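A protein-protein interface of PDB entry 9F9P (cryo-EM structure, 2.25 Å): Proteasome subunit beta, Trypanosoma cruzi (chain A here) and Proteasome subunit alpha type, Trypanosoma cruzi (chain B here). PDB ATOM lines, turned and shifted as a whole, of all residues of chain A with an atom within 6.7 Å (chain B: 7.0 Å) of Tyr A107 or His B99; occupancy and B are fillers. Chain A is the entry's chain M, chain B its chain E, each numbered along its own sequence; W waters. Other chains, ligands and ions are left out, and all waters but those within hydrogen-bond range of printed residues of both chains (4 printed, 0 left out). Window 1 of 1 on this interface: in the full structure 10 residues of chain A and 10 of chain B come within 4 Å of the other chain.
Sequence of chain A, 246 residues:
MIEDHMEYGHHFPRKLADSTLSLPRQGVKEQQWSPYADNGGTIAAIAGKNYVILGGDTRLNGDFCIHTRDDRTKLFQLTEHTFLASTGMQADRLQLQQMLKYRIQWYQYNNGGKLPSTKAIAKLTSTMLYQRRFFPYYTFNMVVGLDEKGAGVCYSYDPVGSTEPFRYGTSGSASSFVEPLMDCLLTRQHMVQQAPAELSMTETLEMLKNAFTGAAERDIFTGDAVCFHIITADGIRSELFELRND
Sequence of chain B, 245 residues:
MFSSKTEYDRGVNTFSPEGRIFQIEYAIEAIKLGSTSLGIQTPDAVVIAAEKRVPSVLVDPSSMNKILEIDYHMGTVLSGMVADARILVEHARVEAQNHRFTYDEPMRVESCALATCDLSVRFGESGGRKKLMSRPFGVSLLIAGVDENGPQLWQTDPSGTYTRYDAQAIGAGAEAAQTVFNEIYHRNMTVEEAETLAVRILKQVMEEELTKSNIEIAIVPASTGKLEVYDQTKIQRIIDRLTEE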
ATOM      1  N   TYR A 102     -31.417   4.149  13.376  1.00  0.00           N
ATOM      2  CA  TYR A 102     -30.513   4.986  14.153  1.00  0.00           C
ATOM      3  C   TYR A 102     -29.248   5.367  13.382  1.00  0.00           C
ATOM      4  O   TYR A 102     -28.914   6.539  13.450  1.00  0.00           O
ATOM      5  CB  TYR A 102     -30.325   4.393  15.558  1.00  0.00           C
ATOM      6  CG  TYR A 102     -31.645   4.505  16.300  1.00  0.00           C
ATOM      7  CD1 TYR A 102     -32.352   5.704  16.272  1.00  0.00           C
ATOM      8  CD2 TYR A 102     -32.275   3.406  16.885  1.00  0.00           C
ATOM      9  CE1 TYR A 102     -33.590   5.836  16.894  1.00  0.00           C
ATOM     10  CE2 TYR A 102     -33.544   3.505  17.458  1.00  0.00           C
ATOM     11  CZ  TYR A 102     -34.194   4.734  17.489  1.00  0.00           C
ATOM     12  OH  TYR A 102     -35.427   4.926  18.057  1.00  0.00           O
ATOM     13  N   ARG A 103     -28.602   4.483  12.608  1.00  0.00           N
ATOM     14  CA  ARG A 103     -27.489   4.908  11.772  1.00  0.00           C
ATOM     15  C   ARG A 103     -27.905   5.957  10.734  1.00  0.00           C
ATOM     16  O   ARG A 103     -27.114   6.851  10.402  1.00  0.00           O
ATOM     17  CB  ARG A 103     -26.818   3.763  11.015  1.00  0.00           C
ATOM     18  CG  ARG A 103     -26.196   2.676  11.879  1.00  0.00           C
ATOM     19  CD  ARG A 103     -24.909   3.038  12.581  1.00  0.00           C
ATOM     20  NE  ARG A 103     -23.875   3.345  11.603  1.00  0.00           N
ATOM     21  CZ  ARG A 103     -22.921   2.487  11.230  1.00  0.00           C
ATOM     22  NH1 ARG A 103     -21.951   2.896  10.431  1.00  0.00           N
ATOM     23  NH2 ARG A 103     -22.944   1.238  11.675  1.00  0.00           N
ATOM     24  N   ILE A 104     -29.141   5.898  10.241  1.00  0.00           N
ATOM     25  CA  ILE A 104     -29.597   6.853   9.251  1.00  0.00           C
ATOM     26  C   ILE A 104     -29.867   8.204   9.898  1.00  0.00           C
ATOM     27  O   ILE A 104     -29.675   9.229   9.270  1.00  0.00           O
ATOM     28  CB  ILE A 104     -30.816   6.283   8.486  1.00  0.00           C
ATOM     29  CG1 ILE A 104     -30.409   5.109   7.589  1.00  0.00           C
ATOM     30  CG2 ILE A 104     -31.536   7.307   7.685  1.00  0.00           C
ATOM     31  CD1 ILE A 104     -31.575   4.276   7.048  1.00  0.00           C
ATOM     32  N   GLN A 105     -30.313   8.210  11.139  1.00  0.00           N
ATOM     33  CA  GLN A 105     -30.507   9.429  11.904  1.00  0.00           C
ATOM     34  C   GLN A 105     -29.178  10.125  12.191  1.00  0.00           C
ATOM     35  O   GLN A 105     -29.064  11.301  11.917  1.00  0.00           O
ATOM     36  CB  GLN A 105     -31.337   9.063  13.136  1.00  0.00           C
ATOM     37  CG  GLN A 105     -31.990  10.228  13.830  1.00  0.00           C
ATOM     38  CD  GLN A 105     -32.623  11.187  12.842  1.00  0.00           C
ATOM     39  OE1 GLN A 105     -33.688  10.914  12.283  1.00  0.00           O
ATOM     40  NE2 GLN A 105     -31.966  12.327  12.615  1.00  0.00           N
ATOM     41  N   TRP A 106     -28.141   9.381  12.603  1.00  0.00           N
ATOM     42  CA  TRP A 106     -26.810   9.928  12.761  1.00  0.00           C
ATOM     43  C   TRP A 106     -26.286  10.502  11.444  1.00  0.00           C
ATOM     44  O   TRP A 106     -25.777  11.613  11.433  1.00  0.00           O
ATOM     45  CB  TRP A 106     -25.829   8.938  13.390  1.00  0.00           C
ATOM     46  CG  TRP A 106     -25.999   8.739  14.870  1.00  0.00           C
ATOM     47  CD1 TRP A 106     -26.411   7.600  15.505  1.00  0.00           C
ATOM     48  CD2 TRP A 106     -25.892   9.724  15.916  1.00  0.00           C
ATOM     49  NE1 TRP A 106     -26.588   7.811  16.850  1.00  0.00           N
ATOM     50  CE2 TRP A 106     -26.260   9.100  17.132  1.00  0.00           C
ATOM     51  CE3 TRP A 106     -25.575  11.083  15.935  1.00  0.00           C
ATOM     52  CZ2 TRP A 106     -26.220   9.748  18.356  1.00  0.00           C
ATOM     53  CZ3 TRP A 106     -25.532  11.731  17.156  1.00  0.00           C
ATOM     54  CH2 TRP A 106     -25.819  11.061  18.345  1.00  0.00           C
ATOM     55  N   TYR A 107     -26.445   9.822  10.307  1.00  0.00           N
ATOM     56  CA  TYR A 107     -26.055  10.388   9.030  1.00  0.00           C
ATOM     57  C   TYR A 107     -26.705  11.741   8.804  1.00  0.00           C
ATOM     58  O   TYR A 107     -26.040  12.649   8.378  1.00  0.00           O
ATOM     59  CB  TYR A 107     -26.358   9.409   7.881  1.00  0.00           C
ATOM     60  CG  TYR A 107     -26.022   9.827   6.464  1.00  0.00           C
ATOM     61  CD1 TYR A 107     -26.729  10.807   5.797  1.00  0.00           C
ATOM     62  CD2 TYR A 107     -24.960   9.250   5.810  1.00  0.00           C
ATOM     63  CE1 TYR A 107     -26.407  11.205   4.504  1.00  0.00           C
ATOM     64  CE2 TYR A 107     -24.636   9.597   4.514  1.00  0.00           C
ATOM     65  CZ  TYR A 107     -25.356  10.575   3.856  1.00  0.00           C
ATOM     66  OH  TYR A 107     -25.004  10.875   2.582  1.00  0.00           O
ATOM     67  N   GLN A 108     -27.975  11.926   9.036  1.00  0.00           N
ATOM     68  CA  GLN A 108     -28.526  13.259   8.860  1.00  0.00           C
ATOM     69  C   GLN A 108     -27.908  14.292   9.819  1.00  0.00           C
ATOM     70  O   GLN A 108     -27.701  15.427   9.442  1.00  0.00           O
ATOM     71  CB  GLN A 108     -30.008  13.320   9.186  1.00  0.00           C
ATOM     72  CG  GLN A 108     -30.892  12.507   8.270  1.00  0.00           C
ATOM     73  CD  GLN A 108     -32.352  12.806   8.555  1.00  0.00           C
ATOM     74  OE1 GLN A 108     -33.057  12.022   9.184  1.00  0.00           O
ATOM     75  NE2 GLN A 108     -32.816  13.956   8.098  1.00  0.00           N
ATOM     76  N   TYR A 109     -27.665  13.964  11.082  1.00  0.00           N
ATOM     77  CA  TYR A 109     -27.092  14.944  11.996  1.00  0.00           C
ATOM     78  C   TYR A 109     -25.676  15.368  11.594  1.00  0.00           C
ATOM     79  O   TYR A 109     -25.310  16.497  11.859  1.00  0.00           O
ATOM     80  CB  TYR A 109     -27.065  14.409  13.426  1.00  0.00           C
ATOM     81  CG  TYR A 109     -28.416  14.243  14.072  1.00  0.00           C
ATOM     82  CD1 TYR A 109     -29.423  15.156  13.863  1.00  0.00           C
ATOM     83  CD2 TYR A 109     -28.654  13.210  14.965  1.00  0.00           C
ATOM     84  CE1 TYR A 109     -30.652  15.021  14.476  1.00  0.00           C
ATOM     85  CE2 TYR A 109     -29.876  13.057  15.606  1.00  0.00           C
ATOM     86  CZ  TYR A 109     -30.870  13.992  15.372  1.00  0.00           C
ATOM     87  OH  TYR A 109     -32.123  13.874  15.924  1.00  0.00           O
ATOM     88  N   ASN A 110     -24.887  14.462  11.005  1.00  0.00           N
ATOM     89  CA  ASN A 110     -23.548  14.735  10.512  1.00  0.00           C
ATOM     90  C   ASN A 110     -23.504  15.221   9.064  1.00  0.00           C
ATOM     91  O   ASN A 110     -22.428  15.513   8.568  1.00  0.00           O
ATOM     92  CB  ASN A 110     -22.671  13.492  10.569  1.00  0.00           C
ATOM     93  CG  ASN A 110     -22.591  12.965  11.980  1.00  0.00           C
ATOM     94  OD1 ASN A 110     -22.689  13.748  12.925  1.00  0.00           O
ATOM     95  ND2 ASN A 110     -22.485  11.649  12.146  1.00  0.00           N
ATOM     96  N   ASN A 111     -24.630  15.333   8.370  1.00  0.00           N
ATOM     97  CA  ASN A 111     -24.585  15.785   6.985  1.00  0.00           C
ATOM     98  C   ASN A 111     -25.615  16.869   6.735  1.00  0.00           C
ATOM     99  O   ASN A 111     -26.215  16.933   5.678  1.00  0.00           O
ATOM    100  CB  ASN A 111     -24.799  14.654   5.971  1.00  0.00           C
ATOM    101  CG  ASN A 111     -23.667  13.651   5.933  1.00  0.00           C
ATOM    102  OD1 ASN A 111     -22.787  13.749   5.090  1.00  0.00           O
ATOM    103  ND2 ASN A 111     -23.665  12.653   6.801  1.00  0.00           N
ATOM    104  N   GLY A 112     -25.820  17.789   7.642  1.00  0.00           N
ATOM    105  CA  GLY A 112     -26.580  18.962   7.237  1.00  0.00           C
ATOM    106  C   GLY A 112     -28.071  18.684   7.044  1.00  0.00           C
ATOM    107  O   GLY A 112     -28.756  19.452   6.379  1.00  0.00           O
ATOM    108  N   GLY A 113     -28.584  17.603   7.641  1.00  0.00           N
ATOM    109  CA  GLY A 113     -30.002  17.311   7.578  1.00  0.00           C
ATOM    110  C   GLY A 113     -30.411  16.416   6.411  1.00  0.00           C
ATOM    111  O   GLY A 113     -31.561  15.979   6.387  1.00  0.00           O
ATOM    112  N   LYS A 114     -29.482  16.104   5.491  1.00  0.00           N
ATOM    113  CA  LYS A 114     -29.778  15.359   4.275  1.00  0.00           C
ATOM    114  C   LYS A 114     -29.826  13.844   4.485  1.00  0.00           C
ATOM    115  O   LYS A 114     -28.999  13.301   5.199  1.00  0.00           O
ATOM    116  CB  LYS A 114     -28.698  15.668   3.230  1.00  0.00           C
ATOM    117  CG  LYS A 114     -29.008  16.909   2.402  1.00  0.00           C
ATOM    118  CD  LYS A 114     -27.789  17.702   1.997  1.00  0.00           C
ATOM    119  CE  LYS A 114     -28.004  19.204   2.057  1.00  0.00           C
ATOM    120  NZ  LYS A 114     -26.942  19.864   2.865  1.00  0.00           N
ATOM    121  N   LEU A 115     -30.681  13.153   3.712  1.00  0.00           N
ATOM    122  CA  LEU A 115     -30.870  11.708   3.814  1.00  0.00           C
ATOM    123  C   LEU A 115     -29.980  10.954   2.853  1.00  0.00           C
ATOM    124  O   LEU A 115     -29.723  11.382   1.749  1.00  0.00           O
ATOM    125  CB  LEU A 115     -32.332  11.378   3.498  1.00  0.00           C
ATOM    126  CG  LEU A 115     -33.326  11.945   4.526  1.00  0.00           C
ATOM    127  CD1 LEU A 115     -34.691  12.121   3.905  1.00  0.00           C
ATOM    128  CD2 LEU A 115     -33.417  11.068   5.770  1.00  0.00           C
ATOM    129  N   PRO A 116     -29.549   9.743   3.215  1.00  0.00           N
ATOM    130  CA  PRO A 116     -28.743   8.922   2.326  1.00  0.00           C
ATOM    131  C   PRO A 116     -29.572   8.336   1.188  1.00  0.00           C
ATOM    132  O   PRO A 116     -30.791   8.163   1.287  1.00  0.00           O
ATOM    133  CB  PRO A 116     -28.142   7.864   3.257  1.00  0.00           C
ATOM    134  CG  PRO A 116     -29.077   7.788   4.421  1.00  0.00           C
ATOM    135  CD  PRO A 116     -29.871   9.080   4.468  1.00  0.00           C
ATOM    136  N   SER A 117     -28.889   8.086   0.065  1.00  0.00           N
ATOM    137  CA  SER A 117     -29.499   7.480  -1.105  1.00  0.00           C
ATOM    138  C   SER A 117     -29.755   5.983  -0.901  1.00  0.00           C
ATOM    139  O   SER A 117     -29.275   5.361   0.036  1.00  0.00           O
ATOM    140  CB  SER A 117     -28.601   7.726  -2.291  1.00  0.00           C
ATOM    141  OG  SER A 117     -27.360   6.988  -2.257  1.00  0.00           O
ATOM    142  N   ALA A 120     -26.320   4.217  -0.976  1.00  0.00           N
ATOM    143  CA  ALA A 120     -25.620   4.399   0.290  1.00  0.00           C
ATOM    144  C   ALA A 120     -26.161   3.526   1.410  1.00  0.00           C
ATOM    145  O   ALA A 120     -25.392   2.933   2.144  1.00  0.00           O
ATOM    146  CB  ALA A 120     -25.685   5.865   0.675  1.00  0.00           C
ATOM    147  N   VAL B  94      -8.326   9.622   7.184  1.00  0.00           N
ATOM    148  CA  VAL B  94      -8.898   8.389   7.678  1.00  0.00           C
ATOM    149  C   VAL B  94     -10.411   8.481   7.749  1.00  0.00           C
ATOM    150  O   VAL B  94     -11.055   7.535   7.312  1.00  0.00           O
ATOM    151  CB  VAL B  94      -8.264   8.005   9.021  1.00  0.00           C
ATOM    152  CG1 VAL B  94      -9.076   6.996   9.806  1.00  0.00           C
ATOM    153  CG2 VAL B  94      -6.840   7.471   8.788  1.00  0.00           C
ATOM    154  N   GLU B  95     -10.978   9.617   8.169  1.00  0.00           N
ATOM    155  CA  GLU B  95     -12.431   9.791   8.138  1.00  0.00           C
ATOM    156  C   GLU B  95     -13.015   9.783   6.722  1.00  0.00           C
ATOM    157  O   GLU B  95     -14.023   9.147   6.495  1.00  0.00           O
ATOM    158  CB  GLU B  95     -12.860  11.066   8.829  1.00  0.00           C
ATOM    159  CG  GLU B  95     -12.658  11.023  10.337  1.00  0.00           C
ATOM    160  CD  GLU B  95     -13.305   9.858  11.069  1.00  0.00           C
ATOM    161  OE1 GLU B  95     -14.360  10.091  11.723  1.00  0.00           O
ATOM    162  OE2 GLU B  95     -12.756   8.719  11.004  1.00  0.00           O
ATOM    163  N   ALA B  96     -12.411  10.467   5.771  1.00  0.00           N
ATOM    164  CA  ALA B  96     -12.946  10.479   4.439  1.00  0.00           C
ATOM    165  C   ALA B  96     -12.925   9.085   3.794  1.00  0.00           C
ATOM    166  O   ALA B  96     -13.797   8.790   2.996  1.00  0.00           O
ATOM    167  CB  ALA B  96     -12.191  11.490   3.611  1.00  0.00           C
ATOM    168  N   GLN B  97     -11.977   8.215   4.133  1.00  0.00           N
ATOM    169  CA  GLN B  97     -11.980   6.856   3.605  1.00  0.00           C
ATOM    170  C   GLN B  97     -12.966   5.934   4.327  1.00  0.00           C
ATOM    171  O   GLN B  97     -13.504   5.043   3.681  1.00  0.00           O
ATOM    172  CB  GLN B  97     -10.599   6.194   3.689  1.00  0.00           C
ATOM    173  CG  GLN B  97      -9.632   6.799   2.702  1.00  0.00           C
ATOM    174  CD  GLN B  97     -10.095   6.669   1.273  1.00  0.00           C
ATOM    175  OE1 GLN B  97     -10.448   5.573   0.809  1.00  0.00           O
ATOM    176  NE2 GLN B  97     -10.119   7.784   0.553  1.00  0.00           N
ATOM    177  N   ASN B  98     -13.176   6.123   5.630  1.00  0.00           N
ATOM    178  CA  ASN B  98     -14.214   5.400   6.341  1.00  0.00           C
ATOM    179  C   ASN B  98     -15.586   5.733   5.759  1.00  0.00           C
ATOM    180  O   ASN B  98     -16.382   4.849   5.566  1.00  0.00           O
ATOM    181  CB  ASN B  98     -14.248   5.710   7.840  1.00  0.00           C
ATOM    182  CG  ASN B  98     -13.094   5.109   8.619  1.00  0.00           C
ATOM    183  OD1 ASN B  98     -12.403   4.193   8.193  1.00  0.00           O
ATOM    184  ND2 ASN B  98     -12.823   5.682   9.781  1.00  0.00           N
ATOM    185  N   HIS B  99     -15.869   6.989   5.444  1.00  0.00           N
ATOM    186  CA  HIS B  99     -17.126   7.313   4.788  1.00  0.00           C
ATOM    187  C   HIS B  99     -17.281   6.587   3.438  1.00  0.00           C
ATOM    188  O   HIS B  99     -18.372   6.133   3.128  1.00  0.00           O
ATOM    189  CB  HIS B  99     -17.251   8.812   4.540  1.00  0.00           C
ATOM    190  CG  HIS B  99     -18.623   9.254   4.214  1.00  0.00           C
ATOM    191  ND1 HIS B  99     -19.542   9.550   5.186  1.00  0.00           N
ATOM    192  CD2 HIS B  99     -19.256   9.453   3.030  1.00  0.00           C
ATOM    193  CE1 HIS B  99     -20.688   9.879   4.580  1.00  0.00           C
ATOM    194  NE2 HIS B  99     -20.557   9.813   3.268  1.00  0.00           N
ATOM    195  N   ARG B 100     -16.237   6.472   2.602  1.00  0.00           N
ATOM    196  CA  ARG B 100     -16.382   5.734   1.352  1.00  0.00           C
ATOM    197  C   ARG B 100     -16.589   4.242   1.558  1.00  0.00           C
ATOM    198  O   ARG B 100     -17.350   3.625   0.833  1.00  0.00           O
ATOM    199  CB  ARG B 100     -15.158   5.823   0.462  1.00  0.00           C
ATOM    200  CG  ARG B 100     -15.019   7.199  -0.121  1.00  0.00           C
ATOM    201  CD  ARG B 100     -14.202   7.166  -1.369  1.00  0.00           C
ATOM    202  NE  ARG B 100     -13.907   8.537  -1.748  1.00  0.00           N
ATOM    203  CZ  ARG B 100     -14.227   9.051  -2.919  1.00  0.00           C
ATOM    204  NH1 ARG B 100     -14.919   8.331  -3.768  1.00  0.00           N
ATOM    205  NH2 ARG B 100     -13.840  10.276  -3.237  1.00  0.00           N
ATOM    206  N   PHE B 101     -15.936   3.701   2.573  1.00  0.00           N
ATOM    207  CA  PHE B 101     -16.021   2.295   2.879  1.00  0.00           C
ATOM    208  C   PHE B 101     -17.450   1.897   3.200  1.00  0.00           C
ATOM    209  O   PHE B 101     -17.987   0.982   2.580  1.00  0.00           O
ATOM    210  CB  PHE B 101     -15.127   1.959   4.057  1.00  0.00           C
ATOM    211  CG  PHE B 101     -15.129   0.497   4.383  1.00  0.00           C
ATOM    212  CD1 PHE B 101     -14.315  -0.380   3.682  1.00  0.00           C
ATOM    213  CD2 PHE B 101     -16.012   0.001   5.329  1.00  0.00           C
ATOM    214  CE1 PHE B 101     -14.361  -1.747   3.945  1.00  0.00           C
ATOM    215  CE2 PHE B 101     -16.095  -1.364   5.564  1.00  0.00           C
ATOM    216  CZ  PHE B 101     -15.280  -2.240   4.862  1.00  0.00           C
ATOM    217  N   THR B 102     -18.091   2.669   4.081  1.00  0.00           N
ATOM    218  CA  THR B 102     -19.392   2.353   4.645  1.00  0.00           C
ATOM    219  C   THR B 102     -20.546   2.742   3.729  1.00  0.00           C
ATOM    220  O   THR B 102     -21.509   2.023   3.701  1.00  0.00           O
ATOM    221  CB  THR B 102     -19.502   2.967   6.035  1.00  0.00           C
ATOM    222  OG1 THR B 102     -18.508   2.359   6.843  1.00  0.00           O
ATOM    223  CG2 THR B 102     -20.819   2.646   6.722  1.00  0.00           C
ATOM    224  N   TYR B 103     -20.457   3.829   2.955  1.00  0.00           N
ATOM    225  CA  TYR B 103     -21.580   4.355   2.209  1.00  0.00           C
ATOM    226  C   TYR B 103     -21.304   4.507   0.719  1.00  0.00           C
ATOM    227  O   TYR B 103     -22.135   5.018  -0.006  1.00  0.00           O
ATOM    228  CB  TYR B 103     -21.943   5.765   2.672  1.00  0.00           C
ATOM    229  CG  TYR B 103     -22.294   5.895   4.132  1.00  0.00           C
ATOM    230  CD1 TYR B 103     -23.512   5.453   4.621  1.00  0.00           C
ATOM    231  CD2 TYR B 103     -21.387   6.403   5.046  1.00  0.00           C
ATOM    232  CE1 TYR B 103     -23.822   5.521   5.981  1.00  0.00           C
ATOM    233  CE2 TYR B 103     -21.669   6.432   6.410  1.00  0.00           C
ATOM    234  CZ  TYR B 103     -22.895   6.011   6.878  1.00  0.00           C
ATOM    235  OH  TYR B 103     -23.211   6.115   8.185  1.00  0.00           O
ATOM    236  N   ASP B 104     -20.139   4.120   0.233  1.00  0.00           N
ATOM    237  CA  ASP B 104     -19.884   4.091  -1.198  1.00  0.00           C
ATOM    238  C   ASP B 104     -20.089   5.449  -1.868  1.00  0.00           C
ATOM    239  O   ASP B 104     -20.541   5.526  -3.008  1.00  0.00           O
ATOM    240  CB  ASP B 104     -20.718   2.984  -1.869  1.00  0.00           C
ATOM    241  CG  ASP B 104     -20.153   2.564  -3.227  1.00  0.00           C
ATOM    242  OD1 ASP B 104     -18.900   2.506  -3.361  1.00  0.00           O
ATOM    243  OD2 ASP B 104     -20.959   2.331  -4.171  1.00  0.00           O
ATOM    244  N   GLU B 105     -19.706   6.535  -1.198  1.00  0.00           N
ATOM    245  CA  GLU B 105     -19.815   7.856  -1.803  1.00  0.00           C
ATOM    246  C   GLU B 105     -18.779   8.788  -1.196  1.00  0.00           C
ATOM    247  O   GLU B 105     -18.364   8.584  -0.075  1.00  0.00           O
ATOM    248  CB  GLU B 105     -21.232   8.396  -1.601  1.00  0.00           C
ATOM    249  CG  GLU B 105     -21.553   8.725  -0.162  1.00  0.00           C
ATOM    250  CD  GLU B 105     -22.975   9.175   0.173  1.00  0.00           C
ATOM    251  OE1 GLU B 105     -23.845   9.193  -0.747  1.00  0.00           O
ATOM    252  OE2 GLU B 105     -23.197   9.551   1.357  1.00  0.00           O
ATOM    253  N   PRO B 106     -18.384   9.894  -1.854  1.00  0.00           N
ATOM    254  CA  PRO B 106     -17.501  10.881  -1.224  1.00  0.00           C
ATOM    255  C   PRO B 106     -18.120  11.618  -0.037  1.00  0.00           C
ATOM    256  O   PRO B 106     -19.308  11.842   0.022  1.00  0.00           O
ATOM    257  CB  PRO B 106     -17.153  11.889  -2.310  1.00  0.00           C
ATOM    258  CG  PRO B 106     -18.002  11.548  -3.487  1.00  0.00           C
ATOM    259  CD  PRO B 106     -18.848  10.326  -3.173  1.00  0.00           C
ATOM    260  N   MET B 107     -17.289  11.966   0.919  1.00  0.00           N
ATOM    261  CA  MET B 107     -17.693  12.704   2.092  1.00  0.00           C
ATOM    262  C   MET B 107     -17.882  14.172   1.732  1.00  0.00           C
ATOM    263  O   MET B 107     -17.083  14.710   0.985  1.00  0.00           O
ATOM    264  CB  MET B 107     -16.548  12.616   3.110  1.00  0.00           C
ATOM    265  CG  MET B 107     -16.954  13.040   4.483  1.00  0.00           C
ATOM    266  SD  MET B 107     -15.630  12.917   5.686  1.00  0.00           S
ATOM    267  CE  MET B 107     -16.640  12.566   7.127  1.00  0.00           C
ATOM    268  N   ARG B 108     -18.915  14.819   2.264  1.00  0.00           N
ATOM    269  CA  ARG B 108     -19.155  16.240   2.057  1.00  0.00           C
ATOM    270  C   ARG B 108     -18.098  17.079   2.771  1.00  0.00           C
ATOM    271  O   ARG B 108     -17.543  16.654   3.783  1.00  0.00           O
ATOM    272  CB  ARG B 108     -20.517  16.644   2.609  1.00  0.00           C
ATOM    273  CG  ARG B 108     -21.703  16.139   1.804  1.00  0.00           C
ATOM    274  CD  ARG B 108     -23.032  16.248   2.581  1.00  0.00           C
ATOM    275  NE  ARG B 108     -24.167  15.936   1.688  1.00  0.00           N
ATOM    276  CZ  ARG B 108     -24.726  14.733   1.560  1.00  0.00           C
ATOM    277  NH1 ARG B 108     -24.455  13.753   2.407  1.00  0.00           N
ATOM    278  NH2 ARG B 108     -25.566  14.505   0.581  1.00  0.00           N
ATOM    279  N   SER B 111     -18.877  18.048   6.403  1.00  0.00           N
ATOM    280  CA  SER B 111     -18.776  16.962   7.370  1.00  0.00           C
ATOM    281  C   SER B 111     -17.319  16.733   7.768  1.00  0.00           C
ATOM    282  O   SER B 111     -17.015  16.373   8.899  1.00  0.00           O
ATOM    283  CB  SER B 111     -19.366  15.662   6.837  1.00  0.00           C
ATOM    284  OG  SER B 111     -20.652  15.857   6.255  1.00  0.00           O
ATOM    285  N   GLU B 148     -22.167  18.345  -3.934  1.00  0.00           N
ATOM    286  CA  GLU B 148     -23.446  18.667  -4.562  1.00  0.00           C
ATOM    287  C   GLU B 148     -23.927  20.114  -4.323  1.00  0.00           C
ATOM    288  O   GLU B 148     -24.713  20.628  -5.119  1.00  0.00           O
ATOM    289  CB  GLU B 148     -24.469  17.664  -4.030  1.00  0.00           C
ATOM    290  CG  GLU B 148     -24.775  17.880  -2.549  1.00  0.00           C
ATOM    291  CD  GLU B 148     -25.374  16.719  -1.775  1.00  0.00           C
ATOM    292  OE1 GLU B 148     -25.393  15.586  -2.306  1.00  0.00           O
ATOM    293  OE2 GLU B 148     -25.833  16.961  -0.638  1.00  0.00           O
HETATM  294  O   HOH W   1     -26.286   9.809  -0.344  1.00  0.00           O
HETATM  295  O   HOH W   2     -24.625   7.589  -2.735  1.00  0.00           O
HETATM  296  O   HOH W   3     -23.434   5.507  -2.384  1.00  0.00           O
HETATM  297  O   HOH W   4     -24.435   6.629  10.610  1.00  0.00           O
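Among the printed residues, pairs that only touch across the chains: Lys A114 with Glu B148 (3.4 Å), Ala A120 with Tyr B103 (3.6 Å), Arg A103 with Thr B102 (3.9 Å), Tyr A107 with Tyr B103 (3.9 Å) and Tyr A107 with His B99 (3.96 Å).
Water W1 lies within hydrogen-bond range of OE1 of Glu B105 (2.5 Å), N of Ser A117 (3.1 Å) and OH of Tyr A107 (3.4 Å). Water W2 lies within hydrogen-bond range of the side-chain carboxylate (OE1) of Glu B105 (2.7 Å) and the side-chain hydroxyl (OG) of Ser A117 (2.8 Å). Water W4 lies within hydrogen-bond range of the backbone carbonyl oxygen of Arg A103 (2.7 Å) and the side-chain hydroxyl of Tyr B103 (2.8 Å). Water W3 lies within hydrogen-bond range of O of Tyr B103, O of Asp B104 and N of Ala A120.
O of Trp A106 sits at hydrogen-bond distance from ND2 of Asn A110. The backbone carbonyl oxygen (O) of Tyr A107 sits at hydrogen-bond distance from the side-chain amide nitrogen (ND2) of Asn A111 (2.9 Å). The backbone NH (N) of Ala A120 is in hydrogen-bond range of the side-chain hydroxyl (OG) of Ser A117, 3.2 Å away. The side-chain carboxylate (OE2) of Glu B105 lies within hydrogen-bond range of a ring nitrogen (NE2) of His B99, at 3.3 Å. The guanidinium group of Arg B108 is in salt-bridge range of the side-chain carboxylate of Glu B148, at 2.8 Å.
Of the 17 printed residues of chain A, 6 touch a printed residue of chain B. Printed residues of chain A that touch a printed residue of chain B: Arg A103, Tyr A107, Asn A110, Asn A111, Lys A114 and Ala A120. Hydrophobic or aromatic side chains of chain A within 4 Å of the printed part of chain B: Tyr A107 and Ala A120.
Of chain B, only His B99, Tyr B103, Glu B105 and Arg B108 come within 4 Å of Tyr A107. Printed residues of chain B within 4 Å of Lys A114: Glu B148. Of the printed residues of chain B, Asn A111 touches Arg B108 (3.2 Å) and Ser B111 (3.2 Å). Printed residues of chain A within 4 Å of Arg B108: Tyr A107 and Asn A111. Ala B96 touches none of the printed residues of chain A.
OH of Tyr A107 is in hydrogen-bond range of OE2 of Glu B105, 2.6 Å away. NH1 of Arg B108 lies within hydrogen-bond range of OH of Tyr A107 (2.9 Å). O of Asn A110 sits at hydrogen-bond distance from OG of Ser B111. The side-chain amide oxygen (OD1) of Asn A111 is in hydrogen-bond range of the guanidinium group (NH1) of Arg B108 (3.2 Å). OG of Ser B111 lies within hydrogen-bond range of OD1 of Asn A111 (3.2 Å).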
